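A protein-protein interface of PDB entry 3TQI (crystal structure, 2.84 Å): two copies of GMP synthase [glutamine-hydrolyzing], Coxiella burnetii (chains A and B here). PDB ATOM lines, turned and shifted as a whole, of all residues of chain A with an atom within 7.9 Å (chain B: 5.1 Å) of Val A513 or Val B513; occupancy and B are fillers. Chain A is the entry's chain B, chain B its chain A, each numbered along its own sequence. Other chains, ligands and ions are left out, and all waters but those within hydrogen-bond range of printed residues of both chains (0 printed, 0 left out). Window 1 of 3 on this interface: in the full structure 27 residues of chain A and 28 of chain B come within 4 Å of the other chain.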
ATOM      1  N   PHE A 433     -26.091  17.237  31.876  1.00  0.00           N
ATOM      2  CA  PHE A 433     -25.817  15.835  31.592  1.00  0.00           C
ATOM      3  C   PHE A 433     -26.434  14.921  32.635  1.00  0.00           C
ATOM      4  O   PHE A 433     -27.055  13.921  32.284  1.00  0.00           O
ATOM      5  CB  PHE A 433     -24.306  15.599  31.488  1.00  0.00           C
ATOM      6  CG  PHE A 433     -23.914  14.196  31.091  1.00  0.00           C
ATOM      7  CD1 PHE A 433     -24.762  13.375  30.370  1.00  0.00           C
ATOM      8  CD2 PHE A 433     -22.653  13.718  31.415  1.00  0.00           C
ATOM      9  CE1 PHE A 433     -24.372  12.100  30.011  1.00  0.00           C
ATOM     10  CE2 PHE A 433     -22.256  12.443  31.052  1.00  0.00           C
ATOM     11  CZ  PHE A 433     -23.119  11.634  30.348  1.00  0.00           C
ATOM     12  N   PHE A 450     -19.705  12.323  33.882  1.00  0.00           N
ATOM     13  CA  PHE A 450     -19.342  13.736  34.002  1.00  0.00           C
ATOM     14  C   PHE A 450     -18.975  14.352  32.657  1.00  0.00           C
ATOM     15  O   PHE A 450     -18.679  13.642  31.703  1.00  0.00           O
ATOM     16  CB  PHE A 450     -18.173  13.914  34.966  1.00  0.00           C
ATOM     17  CG  PHE A 450     -16.945  13.142  34.583  1.00  0.00           C
ATOM     18  CD1 PHE A 450     -16.034  13.659  33.675  1.00  0.00           C
ATOM     19  CD2 PHE A 450     -16.690  11.903  35.145  1.00  0.00           C
ATOM     20  CE1 PHE A 450     -14.894  12.948  33.330  1.00  0.00           C
ATOM     21  CE2 PHE A 450     -15.553  11.186  34.799  1.00  0.00           C
ATOM     22  CZ  PHE A 450     -14.655  11.714  33.892  1.00  0.00           C
ATOM     23  N   ALA A 451     -18.984  15.678  32.599  1.00  0.00           N
ATOM     24  CA  ALA A 451     -18.529  16.399  31.425  1.00  0.00           C
ATOM     25  C   ALA A 451     -17.090  16.859  31.614  1.00  0.00           C
ATOM     26  O   ALA A 451     -16.623  17.013  32.740  1.00  0.00           O
ATOM     27  CB  ALA A 451     -19.422  17.589  31.168  1.00  0.00           C
ATOM     28  N   VAL A 452     -16.390  17.064  30.503  1.00  0.00           N
ATOM     29  CA  VAL A 452     -15.098  17.739  30.507  1.00  0.00           C
ATOM     30  C   VAL A 452     -15.097  18.836  29.444  1.00  0.00           C
ATOM     31  O   VAL A 452     -15.731  18.704  28.405  1.00  0.00           O
ATOM     32  CB  VAL A 452     -13.923  16.770  30.263  1.00  0.00           C
ATOM     33  CG1 VAL A 452     -13.893  15.696  31.319  1.00  0.00           C
ATOM     34  CG2 VAL A 452     -14.020  16.139  28.900  1.00  0.00           C
ATOM     35  N   MET A 454     -13.107  21.209  26.802  1.00  0.00           N
ATOM     36  CA  MET A 454     -11.919  21.344  25.961  1.00  0.00           C
ATOM     37  C   MET A 454     -11.875  22.757  25.412  1.00  0.00           C
ATOM     38  O   MET A 454     -12.827  23.189  24.755  1.00  0.00           O
ATOM     39  CB  MET A 454     -11.972  20.358  24.811  1.00  0.00           C
ATOM     40  CG  MET A 454     -12.437  18.990  25.222  1.00  0.00           C
ATOM     41  SD  MET A 454     -12.137  17.804  23.939  1.00  0.00           S
ATOM     42  CE  MET A 454     -13.374  16.609  24.354  1.00  0.00           C
ATOM     43  N   ILE A 471     -15.634  22.992  22.845  1.00  0.00           N
ATOM     44  CA  ILE A 471     -16.119  21.618  22.715  1.00  0.00           C
ATOM     45  C   ILE A 471     -16.238  20.965  24.089  1.00  0.00           C
ATOM     46  O   ILE A 471     -15.372  21.153  24.946  1.00  0.00           O
ATOM     47  CB  ILE A 471     -15.174  20.767  21.836  1.00  0.00           C
ATOM     48  CG1 ILE A 471     -14.731  21.560  20.604  1.00  0.00           C
ATOM     49  CG2 ILE A 471     -15.851  19.462  21.431  1.00  0.00           C
ATOM     50  CD1 ILE A 471     -13.810  20.792  19.680  1.00  0.00           C
ATOM     51  N   ILE A 472     -17.308  20.195  24.283  1.00  0.00           N
ATOM     52  CA  ILE A 472     -17.550  19.500  25.537  1.00  0.00           C
ATOM     53  C   ILE A 472     -17.524  17.989  25.351  1.00  0.00           C
ATOM     54  O   ILE A 472     -18.291  17.449  24.566  1.00  0.00           O
ATOM     55  CB  ILE A 472     -18.914  19.872  26.106  1.00  0.00           C
ATOM     56  CG1 ILE A 472     -18.879  21.284  26.678  1.00  0.00           C
ATOM     57  CG2 ILE A 472     -19.321  18.883  27.189  1.00  0.00           C
ATOM     58  CD1 ILE A 472     -18.059  21.409  27.956  1.00  0.00           C
ATOM     59  N   ALA A 473     -16.651  17.308  26.083  1.00  0.00           N
ATOM     60  CA  ALA A 473     -16.614  15.851  26.066  1.00  0.00           C
ATOM     61  C   ALA A 473     -17.443  15.324  27.219  1.00  0.00           C
ATOM     62  O   ALA A 473     -17.430  15.903  28.297  1.00  0.00           O
ATOM     63  CB  ALA A 473     -15.197  15.361  26.188  1.00  0.00           C
ATOM     64  N   LEU A 474     -18.159  14.227  26.989  1.00  0.00           N
ATOM     65  CA  LEU A 474     -18.923  13.569  28.037  1.00  0.00           C
ATOM     66  C   LEU A 474     -18.340  12.205  28.302  1.00  0.00           C
ATOM     67  O   LEU A 474     -17.989  11.479  27.380  1.00  0.00           O
ATOM     68  CB  LEU A 474     -20.377  13.419  27.631  1.00  0.00           C
ATOM     69  CG  LEU A 474     -21.142  14.731  27.506  1.00  0.00           C
ATOM     70  CD1 LEU A 474     -22.562  14.457  27.040  1.00  0.00           C
ATOM     71  CD2 LEU A 474     -21.143  15.481  28.824  1.00  0.00           C
ATOM     72  N   ARG A 475     -18.250  11.862  29.578  1.00  0.00           N
ATOM     73  CA  ARG A 475     -17.631  10.627  30.015  1.00  0.00           C
ATOM     74  C   ARG A 475     -18.621   9.858  30.868  1.00  0.00           C
ATOM     75  O   ARG A 475     -19.203  10.414  31.790  1.00  0.00           O
ATOM     76  CB  ARG A 475     -16.382  10.955  30.827  1.00  0.00           C
ATOM     77  CG  ARG A 475     -15.572   9.761  31.288  1.00  0.00           C
ATOM     78  CD  ARG A 475     -15.214   8.847  30.139  1.00  0.00           C
ATOM     79  NE  ARG A 475     -14.083   7.982  30.463  1.00  0.00           N
ATOM     80  CZ  ARG A 475     -13.734   6.900  29.772  1.00  0.00           C
ATOM     81  NH1 ARG A 475     -14.429   6.522  28.700  1.00  0.00           N
ATOM     82  NH2 ARG A 475     -12.682   6.186  30.157  1.00  0.00           N
ATOM     83  N   SER A 499     -26.894  16.130  24.083  1.00  0.00           N
ATOM     84  CA  SER A 499     -25.988  16.957  23.271  1.00  0.00           C
ATOM     85  C   SER A 499     -26.674  18.172  22.638  1.00  0.00           C
ATOM     86  O   SER A 499     -26.134  19.281  22.683  1.00  0.00           O
ATOM     87  CB  SER A 499     -25.330  16.117  22.179  1.00  0.00           C
ATOM     88  OG  SER A 499     -26.289  15.680  21.239  1.00  0.00           O
ATOM     89  N   ILE A 502     -27.048  20.664  25.444  1.00  0.00           N
ATOM     90  CA  ILE A 502     -25.813  21.329  25.863  1.00  0.00           C
ATOM     91  C   ILE A 502     -25.401  22.428  24.885  1.00  0.00           C
ATOM     92  O   ILE A 502     -24.944  23.482  25.311  1.00  0.00           O
ATOM     93  CB  ILE A 502     -24.628  20.360  26.050  1.00  0.00           C
ATOM     94  CG1 ILE A 502     -24.933  19.312  27.119  1.00  0.00           C
ATOM     95  CG2 ILE A 502     -23.381  21.126  26.491  1.00  0.00           C
ATOM     96  CD1 ILE A 502     -23.752  18.398  27.420  1.00  0.00           C
ATOM     97  N   VAL A 503     -25.564  22.189  23.587  1.00  0.00           N
ATOM     98  CA  VAL A 503     -25.137  23.165  22.573  1.00  0.00           C
ATOM     99  C   VAL A 503     -26.131  24.320  22.387  1.00  0.00           C
ATOM    100  O   VAL A 503     -25.726  25.450  22.110  1.00  0.00           O
ATOM    101  CB  VAL A 503     -24.851  22.478  21.212  1.00  0.00           C
ATOM    102  CG1 VAL A 503     -24.569  23.506  20.116  1.00  0.00           C
ATOM    103  CG2 VAL A 503     -23.685  21.527  21.354  1.00  0.00           C
ATOM    104  N   SER A 510     -21.263  25.047  20.851  1.00  0.00           N
ATOM    105  CA  SER A 510     -21.166  24.431  19.513  1.00  0.00           C
ATOM    106  C   SER A 510     -20.462  23.079  19.554  1.00  0.00           C
ATOM    107  O   SER A 510     -19.259  23.018  19.781  1.00  0.00           O
ATOM    108  CB  SER A 510     -20.394  25.338  18.536  1.00  0.00           C
ATOM    109  OG  SER A 510     -18.985  25.114  18.607  1.00  0.00           O
ATOM    110  N   ARG A 511     -21.206  22.007  19.310  1.00  0.00           N
ATOM    111  CA  ARG A 511     -20.647  20.649  19.235  1.00  0.00           C
ATOM    112  C   ARG A 511     -20.239  20.054  20.592  1.00  0.00           C
ATOM    113  O   ARG A 511     -19.790  20.756  21.485  1.00  0.00           O
ATOM    114  CB  ARG A 511     -19.502  20.581  18.199  1.00  0.00           C
ATOM    115  CG  ARG A 511     -18.656  19.318  18.234  1.00  0.00           C
ATOM    116  CD  ARG A 511     -17.791  19.139  16.981  1.00  0.00           C
ATOM    117  NE  ARG A 511     -17.902  20.242  16.029  1.00  0.00           N
ATOM    118  CZ  ARG A 511     -18.483  20.166  14.834  1.00  0.00           C
ATOM    119  NH1 ARG A 511     -19.012  19.032  14.389  1.00  0.00           N
ATOM    120  NH2 ARG A 511     -18.527  21.242  14.061  1.00  0.00           N
ATOM    121  N   VAL A 512     -20.439  18.746  20.721  1.00  0.00           N
ATOM    122  CA  VAL A 512     -20.133  17.990  21.937  1.00  0.00           C
ATOM    123  C   VAL A 512     -19.871  16.529  21.583  1.00  0.00           C
ATOM    124  O   VAL A 512     -20.549  15.963  20.734  1.00  0.00           O
ATOM    125  CB  VAL A 512     -21.284  18.066  22.968  1.00  0.00           C
ATOM    126  CG1 VAL A 512     -22.578  18.456  22.304  1.00  0.00           C
ATOM    127  CG2 VAL A 512     -21.446  16.745  23.702  1.00  0.00           C
ATOM    128  N   VAL A 513     -18.887  15.924  22.245  1.00  0.00           N
ATOM    129  CA  VAL A 513     -18.438  14.568  21.927  1.00  0.00           C
ATOM    130  C   VAL A 513     -18.554  13.625  23.122  1.00  0.00           C
ATOM    131  O   VAL A 513     -18.836  14.057  24.248  1.00  0.00           O
ATOM    132  CB  VAL A 513     -16.978  14.572  21.467  1.00  0.00           C
ATOM    133  CG1 VAL A 513     -16.815  15.487  20.260  1.00  0.00           C
ATOM    134  CG2 VAL A 513     -16.063  15.003  22.611  1.00  0.00           C
ATOM    135  N   TYR A 514     -18.311  12.339  22.860  1.00  0.00           N
ATOM    136  CA  TYR A 514     -18.480  11.278  23.855  1.00  0.00           C
ATOM    137  C   TYR A 514     -17.282  10.331  23.848  1.00  0.00           C
ATOM    138  O   TYR A 514     -16.880   9.829  22.799  1.00  0.00           O
ATOM    139  CB  TYR A 514     -19.764  10.517  23.535  1.00  0.00           C
ATOM    140  CG  TYR A 514     -20.201   9.476  24.543  1.00  0.00           C
ATOM    141  CD1 TYR A 514     -20.469   9.818  25.854  1.00  0.00           C
ATOM    142  CD2 TYR A 514     -20.394   8.158  24.164  1.00  0.00           C
ATOM    143  CE1 TYR A 514     -20.886   8.869  26.768  1.00  0.00           C
ATOM    144  CE2 TYR A 514     -20.812   7.209  25.067  1.00  0.00           C
ATOM    145  CZ  TYR A 514     -21.054   7.566  26.367  1.00  0.00           C
ATOM    146  OH  TYR A 514     -21.468   6.609  27.265  1.00  0.00           O
ATOM    147  N   ASP A 515     -16.728  10.084  25.031  1.00  0.00           N
ATOM    148  CA  ASP A 515     -15.546   9.241  25.181  1.00  0.00           C
ATOM    149  C   ASP A 515     -15.897   7.776  24.963  1.00  0.00           C
ATOM    150  O   ASP A 515     -16.767   7.241  25.642  1.00  0.00           O
ATOM    151  CB  ASP A 515     -14.962   9.426  26.585  1.00  0.00           C
ATOM    152  CG  ASP A 515     -13.590   8.794  26.749  1.00  0.00           C
ATOM    153  OD1 ASP A 515     -13.166   7.980  25.902  1.00  0.00           O
ATOM    154  OD2 ASP A 515     -12.928   9.111  27.753  1.00  0.00           O
ATOM    155  N   MET A 516     -15.199   7.139  24.027  1.00  0.00           N
ATOM    156  CA  MET A 516     -15.396   5.730  23.711  1.00  0.00           C
ATOM    157  C   MET A 516     -14.168   4.904  24.072  1.00  0.00           C
ATOM    158  O   MET A 516     -13.730   4.067  23.286  1.00  0.00           O
ATOM    159  CB  MET A 516     -15.641   5.559  22.214  1.00  0.00           C
ATOM    160  CG  MET A 516     -16.793   6.347  21.651  1.00  0.00           C
ATOM    161  SD  MET A 516     -17.107   5.845  19.949  1.00  0.00           S
ATOM    162  CE  MET A 516     -15.543   6.231  19.157  1.00  0.00           C
ATOM    163  N   THR A 517     -13.608   5.124  25.253  1.00  0.00           N
ATOM    164  CA  THR A 517     -12.362   4.460  25.619  1.00  0.00           C
ATOM    165  C   THR A 517     -12.474   3.804  26.992  1.00  0.00           C
ATOM    166  O   THR A 517     -13.001   4.403  27.923  1.00  0.00           O
ATOM    167  CB  THR A 517     -11.209   5.459  25.580  1.00  0.00           C
ATOM    168  OG1 THR A 517     -11.278   6.201  24.354  1.00  0.00           O
ATOM    169  CG2 THR A 517      -9.879   4.741  25.653  1.00  0.00           C
ATOM    170  N   TRP A 526      -9.953  12.303  33.080  1.00  0.00           N
ATOM    171  CA  TRP A 526      -8.973  12.814  32.116  1.00  0.00           C
ATOM    172  C   TRP A 526      -7.849  13.514  32.875  1.00  0.00           C
ATOM    173  O   TRP A 526      -6.890  14.000  32.289  1.00  0.00           O
ATOM    174  CB  TRP A 526      -9.637  13.789  31.126  1.00  0.00           C
ATOM    175  CG  TRP A 526     -10.677  13.168  30.183  1.00  0.00           C
ATOM    176  CD1 TRP A 526     -11.446  12.062  30.416  1.00  0.00           C
ATOM    177  CD2 TRP A 526     -11.069  13.651  28.887  1.00  0.00           C
ATOM    178  NE1 TRP A 526     -12.271  11.819  29.345  1.00  0.00           N
ATOM    179  CE2 TRP A 526     -12.062  12.780  28.397  1.00  0.00           C
ATOM    180  CE3 TRP A 526     -10.673  14.734  28.094  1.00  0.00           C
ATOM    181  CZ2 TRP A 526     -12.664  12.956  27.156  1.00  0.00           C
ATOM    182  CZ3 TRP A 526     -11.275  14.910  26.857  1.00  0.00           C
ATOM    183  CH2 TRP A 526     -12.254  14.023  26.399  1.00  0.00           C
ATOM    184  N   MET B 454      -7.302  16.562  17.792  1.00  0.00           N
ATOM    185  CA  MET B 454      -7.277  17.670  18.740  1.00  0.00           C
ATOM    186  C   MET B 454      -5.922  17.638  19.439  1.00  0.00           C
ATOM    187  O   MET B 454      -5.531  16.602  19.978  1.00  0.00           O
ATOM    188  CB  MET B 454      -8.389  17.518  19.778  1.00  0.00           C
ATOM    189  CG  MET B 454      -9.692  16.917  19.259  1.00  0.00           C
ATOM    190  SD  MET B 454     -11.046  17.201  20.400  1.00  0.00           S
ATOM    191  CE  MET B 454     -11.894  15.650  20.285  1.00  0.00           C
ATOM    192  N   ILE B 471      -5.777  13.525  21.621  1.00  0.00           N
ATOM    193  CA  ILE B 471      -7.136  13.016  21.527  1.00  0.00           C
ATOM    194  C   ILE B 471      -7.578  13.007  20.069  1.00  0.00           C
ATOM    195  O   ILE B 471      -7.314  13.958  19.324  1.00  0.00           O
ATOM    196  CB  ILE B 471      -8.128  13.862  22.351  1.00  0.00           C
ATOM    197  CG1 ILE B 471      -7.456  14.377  23.642  1.00  0.00           C
ATOM    198  CG2 ILE B 471      -9.353  13.024  22.714  1.00  0.00           C
ATOM    199  CD1 ILE B 471      -8.423  15.060  24.576  1.00  0.00           C
ATOM    200  N   ILE B 472      -8.240  11.924  19.668  1.00  0.00           N
ATOM    201  CA  ILE B 472      -8.796  11.795  18.331  1.00  0.00           C
ATOM    202  C   ILE B 472     -10.305  11.848  18.442  1.00  0.00           C
ATOM    203  O   ILE B 472     -10.877  11.248  19.338  1.00  0.00           O
ATOM    204  CB  ILE B 472      -8.405  10.455  17.688  1.00  0.00           C
ATOM    205  CG1 ILE B 472      -6.925  10.453  17.307  1.00  0.00           C
ATOM    206  CG2 ILE B 472      -9.263  10.187  16.457  1.00  0.00           C
ATOM    207  CD1 ILE B 472      -6.602  11.362  16.145  1.00  0.00           C
ATOM    208  N   ALA B 473     -10.950  12.581  17.549  1.00  0.00           N
ATOM    209  CA  ALA B 473     -12.402  12.594  17.483  1.00  0.00           C
ATOM    210  C   ALA B 473     -12.838  11.895  16.206  1.00  0.00           C
ATOM    211  O   ALA B 473     -12.232  12.087  15.152  1.00  0.00           O
ATOM    212  CB  ALA B 473     -12.936  14.019  17.525  1.00  0.00           C
ATOM    213  N   LEU B 474     -13.881  11.082  16.308  1.00  0.00           N
ATOM    214  CA  LEU B 474     -14.446  10.404  15.159  1.00  0.00           C
ATOM    215  C   LEU B 474     -15.758  11.069  14.747  1.00  0.00           C
ATOM    216  O   LEU B 474     -16.586  11.402  15.579  1.00  0.00           O
ATOM    217  CB  LEU B 474     -14.659   8.922  15.465  1.00  0.00           C
ATOM    218  CG  LEU B 474     -13.389   8.091  15.652  1.00  0.00           C
ATOM    219  CD1 LEU B 474     -13.720   6.611  15.653  1.00  0.00           C
ATOM    220  CD2 LEU B 474     -12.363   8.377  14.578  1.00  0.00           C
ATOM    221  N   ARG B 511      -7.011   7.607  24.265  1.00  0.00           N
ATOM    222  CA  ARG B 511      -8.393   8.116  24.251  1.00  0.00           C
ATOM    223  C   ARG B 511      -8.880   8.689  22.897  1.00  0.00           C
ATOM    224  O   ARG B 511      -8.235   9.539  22.295  1.00  0.00           O
ATOM    225  CB  ARG B 511      -8.600   9.102  25.418  1.00  0.00           C
ATOM    226  CG  ARG B 511      -9.799  10.011  25.312  1.00  0.00           C
ATOM    227  CD  ARG B 511     -10.158  10.647  26.651  1.00  0.00           C
ATOM    228  NE  ARG B 511      -9.167  10.411  27.704  1.00  0.00           N
ATOM    229  CZ  ARG B 511      -9.367   9.694  28.810  1.00  0.00           C
ATOM    230  NH1 ARG B 511     -10.536   9.119  29.065  1.00  0.00           N
ATOM    231  NH2 ARG B 511      -8.375   9.555  29.682  1.00  0.00           N
ATOM    232  N   VAL B 512     -10.023   8.184  22.434  1.00  0.00           N
ATOM    233  CA  VAL B 512     -10.714   8.697  21.243  1.00  0.00           C
ATOM    234  C   VAL B 512     -12.166   9.036  21.600  1.00  0.00           C
ATOM    235  O   VAL B 512     -12.744   8.444  22.525  1.00  0.00           O
ATOM    236  CB  VAL B 512     -10.721   7.668  20.081  1.00  0.00           C
ATOM    237  CG1 VAL B 512     -11.709   6.575  20.344  1.00  0.00           C
ATOM    238  CG2 VAL B 512     -11.087   8.317  18.793  1.00  0.00           C
ATOM    239  N   VAL B 513     -12.746   9.988  20.869  1.00  0.00           N
ATOM    240  CA  VAL B 513     -14.116  10.432  21.117  1.00  0.00           C
ATOM    241  C   VAL B 513     -14.944  10.474  19.834  1.00  0.00           C
ATOM    242  O   VAL B 513     -14.409  10.446  18.741  1.00  0.00           O
ATOM    243  CB  VAL B 513     -14.151  11.810  21.798  1.00  0.00           C
ATOM    244  CG1 VAL B 513     -13.587  11.714  23.215  1.00  0.00           C
ATOM    245  CG2 VAL B 513     -13.397  12.836  20.969  1.00  0.00           C
ATOM    246  N   TYR B 514     -16.260  10.546  19.994  1.00  0.00           N
ATOM    247  CA  TYR B 514     -17.203  10.436  18.893  1.00  0.00           C
ATOM    248  C   TYR B 514     -18.137  11.628  18.925  1.00  0.00           C
ATOM    249  O   TYR B 514     -18.766  11.904  19.951  1.00  0.00           O
ATOM    250  CB  TYR B 514     -18.002   9.144  19.052  1.00  0.00           C
ATOM    251  CG  TYR B 514     -18.883   8.751  17.879  1.00  0.00           C
ATOM    252  CD1 TYR B 514     -18.363   8.614  16.613  1.00  0.00           C
ATOM    253  CD2 TYR B 514     -20.230   8.464  18.061  1.00  0.00           C
ATOM    254  CE1 TYR B 514     -19.165   8.236  15.551  1.00  0.00           C
ATOM    255  CE2 TYR B 514     -21.036   8.087  17.007  1.00  0.00           C
ATOM    256  CZ  TYR B 514     -20.500   7.974  15.755  1.00  0.00           C
ATOM    257  OH  TYR B 514     -21.294   7.594  14.695  1.00  0.00           O
ATOM    258  N   ASP B 515     -18.222  12.329  17.802  1.00  0.00           N
ATOM    259  CA  ASP B 515     -19.074  13.501  17.681  1.00  0.00           C
ATOM    260  C   ASP B 515     -20.537  13.088  17.700  1.00  0.00           C
ATOM    261  O   ASP B 515     -20.932  12.206  16.940  1.00  0.00           O
ATOM    262  CB  ASP B 515     -18.768  14.231  16.375  1.00  0.00           C
ATOM    263  CG  ASP B 515     -19.395  15.613  16.309  1.00  0.00           C
ATOM    264  OD1 ASP B 515     -20.419  15.858  16.990  1.00  0.00           O
ATOM    265  OD2 ASP B 515     -18.858  16.456  15.556  1.00  0.00           O
ATOM    266  N   MET B 516     -21.322  13.741  18.560  1.00  0.00           N
ATOM    267  CA  MET B 516     -22.754  13.469  18.715  1.00  0.00           C
ATOM    268  C   MET B 516     -23.599  14.692  18.367  1.00  0.00           C
ATOM    269  O   MET B 516     -24.610  14.942  19.016  1.00  0.00           O
ATOM    270  CB  MET B 516     -23.079  13.103  20.170  1.00  0.00           C
ATOM    271  CG  MET B 516     -22.235  12.024  20.803  1.00  0.00           C
ATOM    272  SD  MET B 516     -22.950  11.525  22.383  1.00  0.00           S
ATOM    273  CE  MET B 516     -23.012  13.080  23.275  1.00  0.00           C
ATOM    274  N   TRP B 526     -15.338  20.038  11.052  1.00  0.00           N
ATOM    275  CA  TRP B 526     -14.980  20.977  12.107  1.00  0.00           C
ATOM    276  C   TRP B 526     -14.179  22.096  11.447  1.00  0.00           C
ATOM    277  O   TRP B 526     -13.961  23.144  12.033  1.00  0.00           O
ATOM    278  CB  TRP B 526     -14.145  20.282  13.192  1.00  0.00           C
ATOM    279  CG  TRP B 526     -14.818  19.089  13.874  1.00  0.00           C
ATOM    280  CD1 TRP B 526     -15.808  18.304  13.368  1.00  0.00           C
ATOM    281  CD2 TRP B 526     -14.511  18.547  15.169  1.00  0.00           C
ATOM    282  NE1 TRP B 526     -16.149  17.328  14.264  1.00  0.00           N
ATOM    283  CE2 TRP B 526     -15.367  17.451  15.377  1.00  0.00           C
ATOM    284  CE3 TRP B 526     -13.595  18.886  16.173  1.00  0.00           C
ATOM    285  CZ2 TRP B 526     -15.339  16.686  16.545  1.00  0.00           C
ATOM    286  CZ3 TRP B 526     -13.567  18.120  17.340  1.00  0.00           C
ATOM    287  CH2 TRP B 526     -14.436  17.033  17.511  1.00  0.00           C
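NE1 of Trp A526 lies close to NH1 of Arg B511 (3.2 Å).
The side-chain hydroxyl (OG) of Ser A499 lies within hydrogen-bond range of the backbone carbonyl oxygen (O) of Met B516 (2.9 Å).
N of Met B516 is in hydrogen-bond range of O of Val A512, 3.2 Å away.
The guanidinium group (NH1) of Arg A511 lies close to the indole nitrogen (NE1) of Trp B526, at 3.3 Å.
OD2 of Asp B515 lies within salt-bridge range of NH1 of Arg A511 (2.8 Å).
The backbone carbonyl oxygen (O) of Val B512 is in hydrogen-bond range of the backbone NH (N) of Met A516.
The guanidinium group of Arg B511 lies within salt-bridge range of the side-chain carboxylate of Asp A515 (2.7 Å).
N of Val B512 sits at hydrogen-bond distance from OG1 of Thr A517, at 3.0 Å.
The side-chain carboxylate (OD1) of Asp A515 lies close to the backbone carbonyl oxygen (O) of Val B512 (3.4 Å).
N of Tyr B514 lies within hydrogen-bond range of O of Tyr A514.
The side-chain sulfur (SD) of Met A454 sits close to the side-chain sulfur (SD) of Met B454 (3.8 Å).
The backbone carbonyl oxygen (O) of Ile A471 is in hydrogen-bond range of the backbone NH (N) of Met A454 (2.9 Å).
O of Val B513 is in hydrogen-bond range of N of Leu B474 (2.6 Å).
O of Ile B471 lies within hydrogen-bond range of N of Met B454 (3.0 Å).
The backbone carbonyl oxygen (O) of Phe A450 sits at hydrogen-bond distance from the backbone NH (N) of Arg A475.
The indole nitrogen of Trp B526 is in hydrogen-bond range of the side-chain carboxylate of Asp B515, at 3.1 Å.
The backbone carbonyl oxygen (O) of Val A513 lies within hydrogen-bond range of the backbone NH (N) of Leu A474 (2.8 Å).
Arg B511 touches Arg A475.
Val A512 touches Asp B515.
Val B513 touches Val A513.
CA of Val A513 touches O of Tyr B514, 3.3 Å away.
CA of Asp B515 touches CG1 of Val A513, 3.96 Å away.
CH2 of Trp B526 touches CG1 of Val A513, 3.95 Å away.
Tyr A514 touches Met B516.
Asp A515 touches Val B513.
Leu B474 touches Met A516.
SD of Met A516 touches CB of Tyr B514, 3.5 Å away.
Val B513 touches three residues of chain A.
Of the printed residues of chain A, Arg B511 touches Arg A475 (3.8 Å), Asp A515 (2.7 Å), Thr A517 (3.5 Å) and Trp A526 (3.2 Å).
Of the printed residues of chain B, Ile A471 touches Trp B526.
Phe A450 touches none of the printed residues of chain B.
Val A452 touches none of the printed residues of chain B.
The nearest residue of chain B that does not touch Val A513 is Met B516 (4.4 Å).
The nearest residue of chain A that does not touch Val B513 is Trp A526 (4.2 Å).
Hydrophobic or aromatic side chains of chain B within 4 Å of the printed part of chain A: Met B454, Ile B471, Leu B474, Val B513, Tyr B514, Met B516 and Trp B526.
Of the 22 printed residues of chain A, 12 touch a printed residue of chain B.
Printed residues of chain A that touch a printed residue of chain B: Met A454, Ile A471, Arg A475, Ser A499, Arg A511, Val A512, Val A513, Tyr A514, Asp A515, Met A516, Thr A517 and Trp A526.
Hydrophobic or aromatic side chains of chain A that line the printed part of chain B: Met A454, Ile A471, Val A513, Tyr A514, Met A516 and Trp A526.
Among the printed residues, Asp or Glu carboxylates within 4 Å of a Lys or Arg side-chain nitrogen of the other chain: Arg A511 with Asp B515 (2.8 Å) and Asp A515 with Arg B511 (2.7 Å).
Val A512 touches Asp B515, and with the chains exchanged Asp A515 touches Val B512.
Val B513 touches its own counterpart, Val A513.
Val A513 touches Tyr B514, and with the chains exchanged Tyr A514 touches Val B513.
Val A513 touches Asp B515, and with the chains exchanged Asp A515 touches Val B513.
Positions printed for both chains: 454, 471, 472, 473, 474, 511, 512, 513, 514, 515, 516 and 526.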
